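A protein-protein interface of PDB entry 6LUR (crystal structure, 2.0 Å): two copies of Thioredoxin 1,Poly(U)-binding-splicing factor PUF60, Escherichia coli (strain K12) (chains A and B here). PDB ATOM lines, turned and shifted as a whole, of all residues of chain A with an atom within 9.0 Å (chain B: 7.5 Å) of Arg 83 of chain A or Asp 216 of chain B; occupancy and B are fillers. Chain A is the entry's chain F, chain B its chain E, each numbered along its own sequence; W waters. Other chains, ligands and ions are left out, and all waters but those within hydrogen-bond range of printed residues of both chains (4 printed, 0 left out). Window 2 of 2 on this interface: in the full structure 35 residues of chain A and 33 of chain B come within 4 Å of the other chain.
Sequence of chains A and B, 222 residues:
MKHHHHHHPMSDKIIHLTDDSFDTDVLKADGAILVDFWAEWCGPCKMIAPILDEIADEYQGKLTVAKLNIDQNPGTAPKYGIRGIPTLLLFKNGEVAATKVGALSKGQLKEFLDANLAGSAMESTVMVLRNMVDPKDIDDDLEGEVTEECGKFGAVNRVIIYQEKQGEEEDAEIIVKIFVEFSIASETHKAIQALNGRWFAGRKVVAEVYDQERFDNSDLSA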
ATOM      1  N   PHE A  37     -33.699  11.719   2.407  1.00  0.00           N
ATOM      2  CA  PHE A  37     -33.152  11.694   3.758  1.00  0.00           C
ATOM      3  C   PHE A  37     -33.483  13.024   4.434  1.00  0.00           C
ATOM      4  O   PHE A  37     -33.155  14.071   3.881  1.00  0.00           O
ATOM      5  CB  PHE A  37     -31.646  11.432   3.740  1.00  0.00           C
ATOM      6  CG  PHE A  37     -31.256  10.080   3.195  1.00  0.00           C
ATOM      7  CD1 PHE A  37     -31.206   8.970   4.025  1.00  0.00           C
ATOM      8  CD2 PHE A  37     -30.963   9.911   1.847  1.00  0.00           C
ATOM      9  CE1 PHE A  37     -30.827   7.731   3.532  1.00  0.00           C
ATOM     10  CE2 PHE A  37     -30.612   8.666   1.349  1.00  0.00           C
ATOM     11  CZ  PHE A  37     -30.520   7.584   2.196  1.00  0.00           C
ATOM     12  N   TRP A  41     -36.569  18.979  12.228  1.00  0.00           N
ATOM     13  CA  TRP A  41     -36.138  20.338  12.521  1.00  0.00           C
ATOM     14  C   TRP A  41     -35.664  21.031  11.248  1.00  0.00           C
ATOM     15  O   TRP A  41     -35.345  22.213  11.250  1.00  0.00           O
ATOM     16  CB  TRP A  41     -35.014  20.272  13.555  1.00  0.00           C
ATOM     17  CG  TRP A  41     -34.128  19.089  13.340  1.00  0.00           C
ATOM     18  CD1 TRP A  41     -34.272  17.839  13.873  1.00  0.00           C
ATOM     19  CD2 TRP A  41     -32.929  19.053  12.536  1.00  0.00           C
ATOM     20  NE1 TRP A  41     -33.255  17.023  13.446  1.00  0.00           N
ATOM     21  CE2 TRP A  41     -32.414  17.737  12.624  1.00  0.00           C
ATOM     22  CE3 TRP A  41     -32.247  20.001  11.751  1.00  0.00           C
ATOM     23  CZ2 TRP A  41     -31.257  17.340  11.942  1.00  0.00           C
ATOM     24  CZ3 TRP A  41     -31.091  19.622  11.105  1.00  0.00           C
ATOM     25  CH2 TRP A  41     -30.618  18.302  11.182  1.00  0.00           C
ATOM     26  N   ILE A  70     -33.595  10.658   9.559  1.00  0.00           N
ATOM     27  CA  ILE A  70     -32.230  10.276   9.926  1.00  0.00           C
ATOM     28  C   ILE A  70     -32.024  10.246  11.443  1.00  0.00           C
ATOM     29  O   ILE A  70     -31.093   9.596  11.923  1.00  0.00           O
ATOM     30  CB  ILE A  70     -31.154  11.076   9.146  1.00  0.00           C
ATOM     31  CG1 ILE A  70     -31.217  12.585   9.409  1.00  0.00           C
ATOM     32  CG2 ILE A  70     -31.249  10.756   7.660  1.00  0.00           C
ATOM     33  CD1 ILE A  70     -29.909  13.305   9.099  1.00  0.00           C
ATOM     34  N   ALA A  77     -28.151   6.296   6.318  1.00  0.00           N
ATOM     35  CA  ALA A  77     -27.579   7.423   5.593  1.00  0.00           C
ATOM     36  C   ALA A  77     -26.047   7.385   5.526  1.00  0.00           C
ATOM     37  O   ALA A  77     -25.479   7.673   4.468  1.00  0.00           O
ATOM     38  CB  ALA A  77     -28.170   8.742   6.057  1.00  0.00           C
ATOM     39  N   PRO A  78     -25.294   7.073   6.615  1.00  0.00           N
ATOM     40  CA  PRO A  78     -23.835   6.936   6.517  1.00  0.00           C
ATOM     41  C   PRO A  78     -23.340   5.951   5.452  1.00  0.00           C
ATOM     42  O   PRO A  78     -22.278   6.143   4.857  1.00  0.00           O
ATOM     43  CB  PRO A  78     -23.460   6.422   7.920  1.00  0.00           C
ATOM     44  CG  PRO A  78     -24.478   7.104   8.788  1.00  0.00           C
ATOM     45  CD  PRO A  78     -25.759   6.943   8.002  1.00  0.00           C
ATOM     46  N   LYS A  79     -24.118   4.910   5.186  1.00  0.00           N
ATOM     47  CA  LYS A  79     -23.710   3.935   4.180  1.00  0.00           C
ATOM     48  C   LYS A  79     -23.869   4.500   2.765  1.00  0.00           C
ATOM     49  O   LYS A  79     -23.500   3.818   1.804  1.00  0.00           O
ATOM     50  CB  LYS A  79     -24.595   2.687   4.228  1.00  0.00           C
ATOM     51  CG  LYS A  79     -24.652   1.952   5.553  1.00  0.00           C
ATOM     52  CD  LYS A  79     -25.944   1.190   5.639  1.00  0.00           C
ATOM     53  CE  LYS A  79     -25.975   0.110   6.691  1.00  0.00           C
ATOM     54  NZ  LYS A  79     -27.289  -0.575   6.646  1.00  0.00           N
ATOM     55  N   TYR A  80     -24.454   5.711   2.625  1.00  0.00           N
ATOM     56  CA  TYR A  80     -24.572   6.360   1.320  1.00  0.00           C
ATOM     57  C   TYR A  80     -23.821   7.693   1.290  1.00  0.00           C
ATOM     58  O   TYR A  80     -23.995   8.468   0.351  1.00  0.00           O
ATOM     59  CB  TYR A  80     -26.042   6.449   0.858  1.00  0.00           C
ATOM     60  CG  TYR A  80     -26.629   5.087   0.575  1.00  0.00           C
ATOM     61  CD1 TYR A  80     -27.185   4.325   1.593  1.00  0.00           C
ATOM     62  CD2 TYR A  80     -26.556   4.524  -0.694  1.00  0.00           C
ATOM     63  CE1 TYR A  80     -27.655   3.045   1.358  1.00  0.00           C
ATOM     64  CE2 TYR A  80     -27.052   3.255  -0.960  1.00  0.00           C
ATOM     65  CZ  TYR A  80     -27.590   2.512   0.076  1.00  0.00           C
ATOM     66  OH  TYR A  80     -28.079   1.262  -0.178  1.00  0.00           O
ATOM     67  N   GLY A  81     -22.966   7.941   2.300  1.00  0.00           N
ATOM     68  CA  GLY A  81     -22.163   9.160   2.364  1.00  0.00           C
ATOM     69  C   GLY A  81     -23.008  10.440   2.408  1.00  0.00           C
ATOM     70  O   GLY A  81     -22.625  11.470   1.859  1.00  0.00           O
ATOM     71  N   ILE A  82     -24.165  10.361   3.072  1.00  0.00           N
ATOM     72  CA  ILE A  82     -25.063  11.480   3.257  1.00  0.00           C
ATOM     73  C   ILE A  82     -24.410  12.424   4.266  1.00  0.00           C
ATOM     74  O   ILE A  82     -23.933  11.969   5.305  1.00  0.00           O
ATOM     75  CB  ILE A  82     -26.427  11.000   3.784  1.00  0.00           C
ATOM     76  CG1 ILE A  82     -27.078  10.002   2.825  1.00  0.00           C
ATOM     77  CG2 ILE A  82     -27.330  12.208   4.122  1.00  0.00           C
ATOM     78  CD1 ILE A  82     -27.217  10.513   1.392  1.00  0.00           C
ATOM     79  N   ARG A  83     -24.456  13.720   3.946  1.00  0.00           N
ATOM     80  CA  ARG A  83     -23.839  14.802   4.699  1.00  0.00           C
ATOM     81  C   ARG A  83     -24.963  15.736   5.150  1.00  0.00           C
ATOM     82  O   ARG A  83     -25.535  15.543   6.222  1.00  0.00           O
ATOM     83  CB  ARG A  83     -22.757  15.480   3.840  1.00  0.00           C
ATOM     84  CG  ARG A  83     -21.528  14.608   3.576  1.00  0.00           C
ATOM     85  CD  ARG A  83     -20.448  15.259   2.730  1.00  0.00           C
ATOM     86  NE  ARG A  83     -19.845  16.331   3.519  1.00  0.00           N
ATOM     87  CZ  ARG A  83     -19.469  17.522   3.076  1.00  0.00           C
ATOM     88  NH1 ARG A  83     -19.587  17.831   1.796  1.00  0.00           N
ATOM     89  NH2 ARG A  83     -18.952  18.392   3.922  1.00  0.00           N
ATOM     90  N   GLY A  84     -25.311  16.724   4.316  1.00  0.00           N
ATOM     91  CA  GLY A  84     -26.420  17.615   4.623  1.00  0.00           C
ATOM     92  C   GLY A  84     -27.769  16.998   4.238  1.00  0.00           C
ATOM     93  O   GLY A  84     -27.817  15.992   3.512  1.00  0.00           O
ATOM     94  N   ILE A  85     -28.860  17.596   4.752  1.00  0.00           N
ATOM     95  CA  ILE A  85     -30.229  17.217   4.423  1.00  0.00           C
ATOM     96  C   ILE A  85     -31.018  18.466   4.037  1.00  0.00           C
ATOM     97  O   ILE A  85     -30.751  19.580   4.505  1.00  0.00           O
ATOM     98  CB  ILE A  85     -30.919  16.464   5.582  1.00  0.00           C
ATOM     99  CG1 ILE A  85     -30.932  17.275   6.887  1.00  0.00           C
ATOM    100  CG2 ILE A  85     -30.365  15.054   5.753  1.00  0.00           C
ATOM    101  CD1 ILE A  85     -31.873  16.732   7.956  1.00  0.00           C
ATOM    102  N   PRO A  86     -32.035  18.338   3.165  1.00  0.00           N
ATOM    103  CA  PRO A  86     -32.398  17.049   2.564  1.00  0.00           C
ATOM    104  C   PRO A  86     -31.428  16.602   1.467  1.00  0.00           C
ATOM    105  O   PRO A  86     -30.768  17.434   0.836  1.00  0.00           O
ATOM    106  CB  PRO A  86     -33.767  17.381   1.948  1.00  0.00           C
ATOM    107  CG  PRO A  86     -33.645  18.839   1.541  1.00  0.00           C
ATOM    108  CD  PRO A  86     -32.885  19.457   2.705  1.00  0.00           C
ATOM    109  N   THR A  87     -31.339  15.279   1.265  1.00  0.00           N
ATOM    110  CA  THR A  87     -30.614  14.697   0.143  1.00  0.00           C
ATOM    111  C   THR A  87     -31.539  13.672  -0.502  1.00  0.00           C
ATOM    112  O   THR A  87     -32.108  12.830   0.202  1.00  0.00           O
ATOM    113  CB  THR A  87     -29.257  14.063   0.528  1.00  0.00           C
ATOM    114  OG1 THR A  87     -28.309  15.043   0.953  1.00  0.00           O
ATOM    115  CG2 THR A  87     -28.605  13.291  -0.613  1.00  0.00           C
ATOM    116  N   LEU A  89     -31.827  10.541  -3.193  1.00  0.00           N
ATOM    117  CA  LEU A  89     -31.102   9.492  -3.905  1.00  0.00           C
ATOM    118  C   LEU A  89     -32.102   8.729  -4.764  1.00  0.00           C
ATOM    119  O   LEU A  89     -33.053   8.161  -4.228  1.00  0.00           O
ATOM    120  CB  LEU A  89     -30.550   8.515  -2.867  1.00  0.00           C
ATOM    121  CG  LEU A  89     -29.047   8.369  -2.738  1.00  0.00           C
ATOM    122  CD1 LEU A  89     -28.414   9.698  -2.293  1.00  0.00           C
ATOM    123  CD2 LEU A  89     -28.767   7.271  -1.718  1.00  0.00           C
ATOM    124  N   THR A  99     -27.989  11.482  -7.325  1.00  0.00           N
ATOM    125  CA  THR A  99     -28.149  12.108  -6.029  1.00  0.00           C
ATOM    126  C   THR A  99     -28.375  13.602  -6.239  1.00  0.00           C
ATOM    127  O   THR A  99     -27.801  14.211  -7.143  1.00  0.00           O
ATOM    128  CB  THR A  99     -26.912  11.897  -5.144  1.00  0.00           C
ATOM    129  OG1 THR A  99     -25.925  12.788  -5.645  1.00  0.00           O
ATOM    130  CG2 THR A  99     -26.312  10.513  -5.230  1.00  0.00           C
ATOM    131  N   VAL A 101     -28.684  17.097  -3.722  1.00  0.00           N
ATOM    132  CA  VAL A 101     -28.391  17.558  -2.375  1.00  0.00           C
ATOM    133  C   VAL A 101     -29.079  18.909  -2.215  1.00  0.00           C
ATOM    134  O   VAL A 101     -28.845  19.804  -3.019  1.00  0.00           O
ATOM    135  CB  VAL A 101     -26.860  17.670  -2.171  1.00  0.00           C
ATOM    136  CG1 VAL A 101     -26.468  18.548  -0.998  1.00  0.00           C
ATOM    137  CG2 VAL A 101     -26.168  16.313  -2.048  1.00  0.00           C
ATOM    138  N   GLY A 102     -29.903  19.057  -1.169  1.00  0.00           N
ATOM    139  CA  GLY A 102     -30.488  20.354  -0.832  1.00  0.00           C
ATOM    140  C   GLY A 102     -31.873  20.482  -1.454  1.00  0.00           C
ATOM    141  O   GLY A 102     -32.176  19.741  -2.390  1.00  0.00           O
ATOM    142  N   MET B 122      -7.497  18.880  -9.364  1.00  0.00           N
ATOM    143  CA  MET B 122      -7.158  18.958  -7.953  1.00  0.00           C
ATOM    144  C   MET B 122      -6.840  17.570  -7.426  1.00  0.00           C
ATOM    145  O   MET B 122      -7.557  16.635  -7.739  1.00  0.00           O
ATOM    146  CB  MET B 122      -8.356  19.504  -7.169  1.00  0.00           C
ATOM    147  CG  MET B 122      -8.027  19.885  -5.732  1.00  0.00           C
ATOM    148  SD  MET B 122      -9.592  19.990  -4.808  1.00  0.00           S
ATOM    149  CE  MET B 122      -9.974  18.241  -4.670  1.00  0.00           C
ATOM    150  N   THR B 125      -8.702  14.539  -1.390  1.00  0.00           N
ATOM    151  CA  THR B 125      -8.495  13.997  -0.056  1.00  0.00           C
ATOM    152  C   THR B 125      -9.152  12.620   0.104  1.00  0.00           C
ATOM    153  O   THR B 125      -9.028  11.974   1.151  1.00  0.00           O
ATOM    154  CB  THR B 125      -9.087  14.909   1.028  1.00  0.00           C
ATOM    155  OG1 THR B 125     -10.513  15.037   0.847  1.00  0.00           O
ATOM    156  CG2 THR B 125      -8.347  16.233   1.147  1.00  0.00           C
ATOM    157  N   VAL B 126      -9.900  12.191  -0.915  1.00  0.00           N
ATOM    158  CA  VAL B 126     -10.658  10.947  -0.811  1.00  0.00           C
ATOM    159  C   VAL B 126      -9.910   9.823  -1.536  1.00  0.00           C
ATOM    160  O   VAL B 126      -9.529   9.974  -2.693  1.00  0.00           O
ATOM    161  CB  VAL B 126     -12.085  11.096  -1.394  1.00  0.00           C
ATOM    162  CG1 VAL B 126     -12.925   9.848  -1.161  1.00  0.00           C
ATOM    163  CG2 VAL B 126     -12.794  12.331  -0.864  1.00  0.00           C
ATOM    164  N   ARG B 158     -13.515  10.459   7.629  1.00  0.00           N
ATOM    165  CA  ARG B 158     -14.677   9.589   7.558  1.00  0.00           C
ATOM    166  C   ARG B 158     -14.361   8.365   6.695  1.00  0.00           C
ATOM    167  O   ARG B 158     -13.593   8.468   5.743  1.00  0.00           O
ATOM    168  CB  ARG B 158     -15.839  10.351   6.895  1.00  0.00           C
ATOM    169  CG  ARG B 158     -17.220   9.795   7.208  1.00  0.00           C
ATOM    170  CD  ARG B 158     -18.318  10.494   6.443  1.00  0.00           C
ATOM    171  NE  ARG B 158     -19.648  10.055   6.886  1.00  0.00           N
ATOM    172  CZ  ARG B 158     -20.801  10.464   6.351  1.00  0.00           C
ATOM    173  NH1 ARG B 158     -20.795  11.341   5.361  1.00  0.00           N
ATOM    174  NH2 ARG B 158     -21.958  10.047   6.840  1.00  0.00           N
ATOM    175  N   ILE B 160     -16.605   5.408   4.458  1.00  0.00           N
ATOM    176  CA  ILE B 160     -17.876   4.862   3.999  1.00  0.00           C
ATOM    177  C   ILE B 160     -17.673   3.452   3.434  1.00  0.00           C
ATOM    178  O   ILE B 160     -16.797   3.242   2.587  1.00  0.00           O
ATOM    179  CB  ILE B 160     -18.547   5.819   3.005  1.00  0.00           C
ATOM    180  CG1 ILE B 160     -18.778   7.187   3.669  1.00  0.00           C
ATOM    181  CG2 ILE B 160     -19.854   5.230   2.463  1.00  0.00           C
ATOM    182  CD1 ILE B 160     -18.952   8.289   2.670  1.00  0.00           C
ATOM    183  N   GLU B 181     -11.816   9.232   3.527  1.00  0.00           N
ATOM    184  CA  GLU B 181     -11.583  10.657   3.357  1.00  0.00           C
ATOM    185  C   GLU B 181     -10.572  11.094   4.412  1.00  0.00           C
ATOM    186  O   GLU B 181     -10.828  10.939   5.611  1.00  0.00           O
ATOM    187  CB  GLU B 181     -12.913  11.397   3.516  1.00  0.00           C
ATOM    188  CG  GLU B 181     -12.817  12.887   3.256  1.00  0.00           C
ATOM    189  CD  GLU B 181     -13.973  13.711   3.814  1.00  0.00           C
ATOM    190  OE1 GLU B 181     -14.808  13.166   4.576  1.00  0.00           O
ATOM    191  OE2 GLU B 181     -14.018  14.916   3.533  1.00  0.00           O
ATOM    192  N   TYR B 210     -10.576   9.417  -5.343  1.00  0.00           N
ATOM    193  CA  TYR B 210     -11.956   9.562  -5.774  1.00  0.00           C
ATOM    194  C   TYR B 210     -12.311  11.050  -5.874  1.00  0.00           C
ATOM    195  O   TYR B 210     -11.992  11.823  -4.970  1.00  0.00           O
ATOM    196  CB  TYR B 210     -12.865   8.778  -4.832  1.00  0.00           C
ATOM    197  CG  TYR B 210     -14.283   8.671  -5.335  1.00  0.00           C
ATOM    198  CD1 TYR B 210     -14.672   7.653  -6.201  1.00  0.00           C
ATOM    199  CD2 TYR B 210     -15.222   9.632  -4.980  1.00  0.00           C
ATOM    200  CE1 TYR B 210     -15.981   7.603  -6.688  1.00  0.00           C
ATOM    201  CE2 TYR B 210     -16.524   9.598  -5.445  1.00  0.00           C
ATOM    202  CZ  TYR B 210     -16.904   8.568  -6.293  1.00  0.00           C
ATOM    203  OH  TYR B 210     -18.191   8.538  -6.708  1.00  0.00           O
ATOM    204  N   ASP B 211     -13.004  11.434  -6.965  1.00  0.00           N
ATOM    205  CA  ASP B 211     -13.344  12.827  -7.212  1.00  0.00           C
ATOM    206  C   ASP B 211     -13.927  13.471  -5.947  1.00  0.00           C
ATOM    207  O   ASP B 211     -14.969  13.065  -5.445  1.00  0.00           O
ATOM    208  CB  ASP B 211     -14.294  12.972  -8.408  1.00  0.00           C
ATOM    209  CG  ASP B 211     -14.543  14.437  -8.750  1.00  0.00           C
ATOM    210  OD1 ASP B 211     -13.759  15.008  -9.519  1.00  0.00           O
ATOM    211  OD2 ASP B 211     -15.479  15.017  -8.191  1.00  0.00           O
ATOM    212  N   GLN B 212     -13.273  14.516  -5.442  1.00  0.00           N
ATOM    213  CA  GLN B 212     -13.675  15.093  -4.162  1.00  0.00           C
ATOM    214  C   GLN B 212     -15.035  15.790  -4.266  1.00  0.00           C
ATOM    215  O   GLN B 212     -15.837  15.764  -3.337  1.00  0.00           O
ATOM    216  CB  GLN B 212     -12.637  16.111  -3.683  1.00  0.00           C
ATOM    217  CG  GLN B 212     -12.914  16.596  -2.274  1.00  0.00           C
ATOM    218  CD  GLN B 212     -11.720  17.333  -1.740  1.00  0.00           C
ATOM    219  OE1 GLN B 212     -10.723  16.717  -1.373  1.00  0.00           O
ATOM    220  NE2 GLN B 212     -11.818  18.658  -1.725  1.00  0.00           N
ATOM    221  N   GLU B 213     -15.263  16.453  -5.392  1.00  0.00           N
ATOM    222  CA  GLU B 213     -16.527  17.139  -5.616  1.00  0.00           C
ATOM    223  C   GLU B 213     -17.713  16.175  -5.575  1.00  0.00           C
ATOM    224  O   GLU B 213     -18.714  16.448  -4.913  1.00  0.00           O
ATOM    225  CB  GLU B 213     -16.484  17.908  -6.924  1.00  0.00           C
ATOM    226  CG  GLU B 213     -17.608  18.920  -6.979  1.00  0.00           C
ATOM    227  CD  GLU B 213     -17.615  19.737  -8.253  1.00  0.00           C
ATOM    228  OE1 GLU B 213     -18.693  20.294  -8.566  1.00  0.00           O
ATOM    229  OE2 GLU B 213     -16.546  19.780  -8.934  1.00  0.00           O
ATOM    230  N   ARG B 214     -17.587  15.045  -6.285  1.00  0.00           N
ATOM    231  CA  ARG B 214     -18.577  13.985  -6.202  1.00  0.00           C
ATOM    232  C   ARG B 214     -18.804  13.527  -4.757  1.00  0.00           C
ATOM    233  O   ARG B 214     -19.949  13.372  -4.318  1.00  0.00           O
ATOM    234  CB  ARG B 214     -18.148  12.765  -7.043  1.00  0.00           C
ATOM    235  CG  ARG B 214     -18.147  12.990  -8.546  1.00  0.00           C
ATOM    236  CD  ARG B 214     -17.991  11.571  -9.077  1.00  0.00           C
ATOM    237  NE  ARG B 214     -17.742  11.454 -10.494  1.00  0.00           N
ATOM    238  CZ  ARG B 214     -18.694  11.300 -11.410  1.00  0.00           C
ATOM    239  NH1 ARG B 214     -18.358  11.205 -12.681  1.00  0.00           N
ATOM    240  NH2 ARG B 214     -19.970  11.249 -11.063  1.00  0.00           N
ATOM    241  N   PHE B 215     -17.713  13.175  -4.061  1.00  0.00           N
ATOM    242  CA  PHE B 215     -17.844  12.656  -2.709  1.00  0.00           C
ATOM    243  C   PHE B 215     -18.562  13.692  -1.839  1.00  0.00           C
ATOM    244  O   PHE B 215     -19.515  13.369  -1.118  1.00  0.00           O
ATOM    245  CB  PHE B 215     -16.453  12.284  -2.185  1.00  0.00           C
ATOM    246  CG  PHE B 215     -16.440  11.652  -0.820  1.00  0.00           C
ATOM    247  CD1 PHE B 215     -16.605  10.285  -0.678  1.00  0.00           C
ATOM    248  CD2 PHE B 215     -16.278  12.426   0.324  1.00  0.00           C
ATOM    249  CE1 PHE B 215     -16.622   9.704   0.578  1.00  0.00           C
ATOM    250  CE2 PHE B 215     -16.300  11.840   1.582  1.00  0.00           C
ATOM    251  CZ  PHE B 215     -16.479  10.482   1.708  1.00  0.00           C
ATOM    252  N   ASP B 216     -18.111  14.953  -1.921  1.00  0.00           N
ATOM    253  CA  ASP B 216     -18.717  16.009  -1.110  1.00  0.00           C
ATOM    254  C   ASP B 216     -20.195  16.154  -1.457  1.00  0.00           C
ATOM    255  O   ASP B 216     -20.958  16.637  -0.626  1.00  0.00           O
ATOM    256  CB  ASP B 216     -18.060  17.386  -1.268  1.00  0.00           C
ATOM    257  CG  ASP B 216     -16.654  17.483  -0.746  1.00  0.00           C
ATOM    258  OD1 ASP B 216     -16.233  16.569  -0.015  1.00  0.00           O
ATOM    259  OD2 ASP B 216     -15.979  18.476  -1.096  1.00  0.00           O
ATOM    260  N   ASN B 217     -20.602  15.711  -2.657  1.00  0.00           N
ATOM    261  CA  ASN B 217     -22.014  15.807  -3.041  1.00  0.00           C
ATOM    262  C   ASN B 217     -22.769  14.490  -2.863  1.00  0.00           C
ATOM    263  O   ASN B 217     -23.879  14.331  -3.378  1.00  0.00           O
ATOM    264  CB  ASN B 217     -22.218  16.411  -4.442  1.00  0.00           C
ATOM    265  CG  ASN B 217     -21.925  17.898  -4.455  1.00  0.00           C
ATOM    266  OD1 ASN B 217     -22.739  18.698  -4.012  1.00  0.00           O
ATOM    267  ND2 ASN B 217     -20.744  18.280  -4.910  1.00  0.00           N
ATOM    268  N   SER B 218     -22.177  13.540  -2.133  1.00  0.00           N
ATOM    269  CA  SER B 218     -22.826  12.265  -1.862  1.00  0.00           C
ATOM    270  C   SER B 218     -23.046  11.453  -3.142  1.00  0.00           C
ATOM    271  O   SER B 218     -24.028  10.706  -3.249  1.00  0.00           O
ATOM    272  CB  SER B 218     -24.095  12.485  -1.096  1.00  0.00           C
ATOM    273  OG  SER B 218     -23.803  13.170   0.110  1.00  0.00           O
ATOM    274  N   ASP B 219     -22.121  11.608  -4.111  1.00  0.00           N
ATOM    275  CA  ASP B 219     -22.147  10.778  -5.316  1.00  0.00           C
ATOM    276  C   ASP B 219     -20.993   9.785  -5.238  1.00  0.00           C
ATOM    277  O   ASP B 219     -19.850  10.156  -5.514  1.00  0.00           O
ATOM    278  CB  ASP B 219     -22.145  11.615  -6.601  1.00  0.00           C
ATOM    279  CG  ASP B 219     -21.854  10.869  -7.901  1.00  0.00           C
ATOM    280  OD1 ASP B 219     -21.981   9.637  -7.955  1.00  0.00           O
ATOM    281  OD2 ASP B 219     -21.528  11.546  -8.874  1.00  0.00           O
ATOM    282  N   LEU B 220     -21.324   8.555  -4.835  1.00  0.00           N
ATOM    283  CA  LEU B 220     -20.332   7.516  -4.635  1.00  0.00           C
ATOM    284  C   LEU B 220     -20.340   6.548  -5.809  1.00  0.00           C
ATOM    285  O   LEU B 220     -19.855   5.427  -5.675  1.00  0.00           O
ATOM    286  CB  LEU B 220     -20.595   6.798  -3.302  1.00  0.00           C
ATOM    287  CG  LEU B 220     -20.623   7.700  -2.058  1.00  0.00           C
ATOM    288  CD1 LEU B 220     -20.806   6.914  -0.756  1.00  0.00           C
ATOM    289  CD2 LEU B 220     -19.401   8.588  -1.973  1.00  0.00           C
HETATM  290  O   HOH W   1     -24.792   8.180  -2.490  1.00  0.00           O
HETATM  291  O   HOH W   2     -20.067  11.708   1.082  1.00  0.00           O
HETATM  292  O   HOH W   3     -17.621  14.090   4.129  1.00  0.00           O
HETATM  293  O   HOH W   4     -25.643  14.690   1.523  1.00  0.00           O
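The backbone NH of Glu 181 of chain B sits at hydrogen-bond distance from the backbone carbonyl oxygen of Arg 158 of chain B. The backbone carbonyl oxygen (O) of Glu 213 of chain B sits at hydrogen-bond distance from the side-chain amide nitrogen (ND2) of Asn 217 of chain B. The backbone carbonyl oxygen of Ala 77 of chain A sits close to the backbone NH of Ile 82 of chain A.
Pro 78 of chain A touches Arg 158 of chain B (CA to NH2, 3.6 Å). Ile 160 of chain B touches Pro 78 of chain A (CG2 to O, 3.5 Å). Lys 79 of chain A touches Ile 160 of chain B. Tyr 80 of chain A touches Leu 220 of chain B (O to CD1, 3.7 Å). Gly 81 of chain A touches Arg 158 of chain B (C to NH1, 3.8 Å). Gly 81 of chain A touches Ile 160 of chain B (CA to CD1, 3.3 Å). Leu 220 of chain B touches Gly 81 of chain A (CD1 to N, 3.9 Å). CG of Arg 83 of chain A touches NH1 of Arg 158 of chain B, at 3.8 Å. Ser 218 of chain B touches Arg 83 of chain A. Asn 217 of chain B touches Val 101 of chain A (O to CG2, 3.3 Å).
The backbone carbonyl oxygen (O) of Ile 82 of chain A sits at hydrogen-bond distance from the guanidinium group (NH2) of Arg 158 of chain B (3.2 Å). The backbone carbonyl oxygen of Asp 216 of chain B lies within hydrogen-bond range of the guanidinium group of Arg 83 of chain A (3.0 Å). The backbone carbonyl oxygen of Asn 217 of chain B is in hydrogen-bond range of the side-chain hydroxyl of Thr 99 of chain A, 3.4 Å away. O of Gly 81 of chain A sits at hydrogen-bond distance from OG of Ser 218 of chain B, 2.7 Å away.
Of the 18 printed residues of chain A, 8 touch a printed residue of chain B. Of the 17 printed residues of chain B, 6 touch a printed residue of chain A. Hydrophobic or aromatic side chains of chain B that line the printed part of chain A: Ile 160 and Leu 220.
No position is printed for both chains.
Of chain B, only Arg 158, Asp 216 and Ser 218 come within 4 Å of Arg 83 of chain A. Asp 216 of chain B touches one residue of chain A. Gly 84 of chain A touches none of the printed residues of chain B. Asn 217 of chain B touches two residues of chain A. Printed residues of chain B within 4 Å of Thr 99 of chain A: Asn 217 and Ser 218. Of the printed residues of chain B, Val 101 of chain A touches Asn 217. Of the printed residues of chain B, Lys 79 of chain A touches Ile 160 (3.97 Å). Printed residues of chain A within 4 Å of Leu 220 of chain B: Tyr 80 and Gly 81. Of the printed residues of chain B, Gly 81 of chain A touches Arg 158, Ile 160, Ser 218 and Leu 220. The nearest residue of chain B that does not touch Arg 83 of chain A is Phe 215 of chain B (4.4 Å). The nearest printed residue of chain B that does not touch Val 101 of chain A is Ser 218 of chain B (4.5 Å).
Water W2 bridges the backbone carbonyl oxygen of Gly 81 of chain A (2.7 Å) and the backbone carbonyl oxygen of Phe 215 of chain B (2.8 Å). Water W1 lies within hydrogen-bond range of O of Ser 218 of chain B and O of Tyr 80 of chain A. Water W4 lies within hydrogen-bond range of the side-chain hydroxyl (OG1) of Thr 87 of chain A (2.7 Å), the side-chain hydroxyl (OG) of Ser 218 of chain B (2.8 Å), the backbone NH (N) of Arg 83 of chain A (2.9 Å) and the backbone carbonyl oxygen (O) of Gly 84 of chain A (3.2 Å). Water W3 bridges the side-chain carboxylate (OE1) of Glu 181 of chain B and the guanidinium group (NE) of Arg 83 of chain A.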
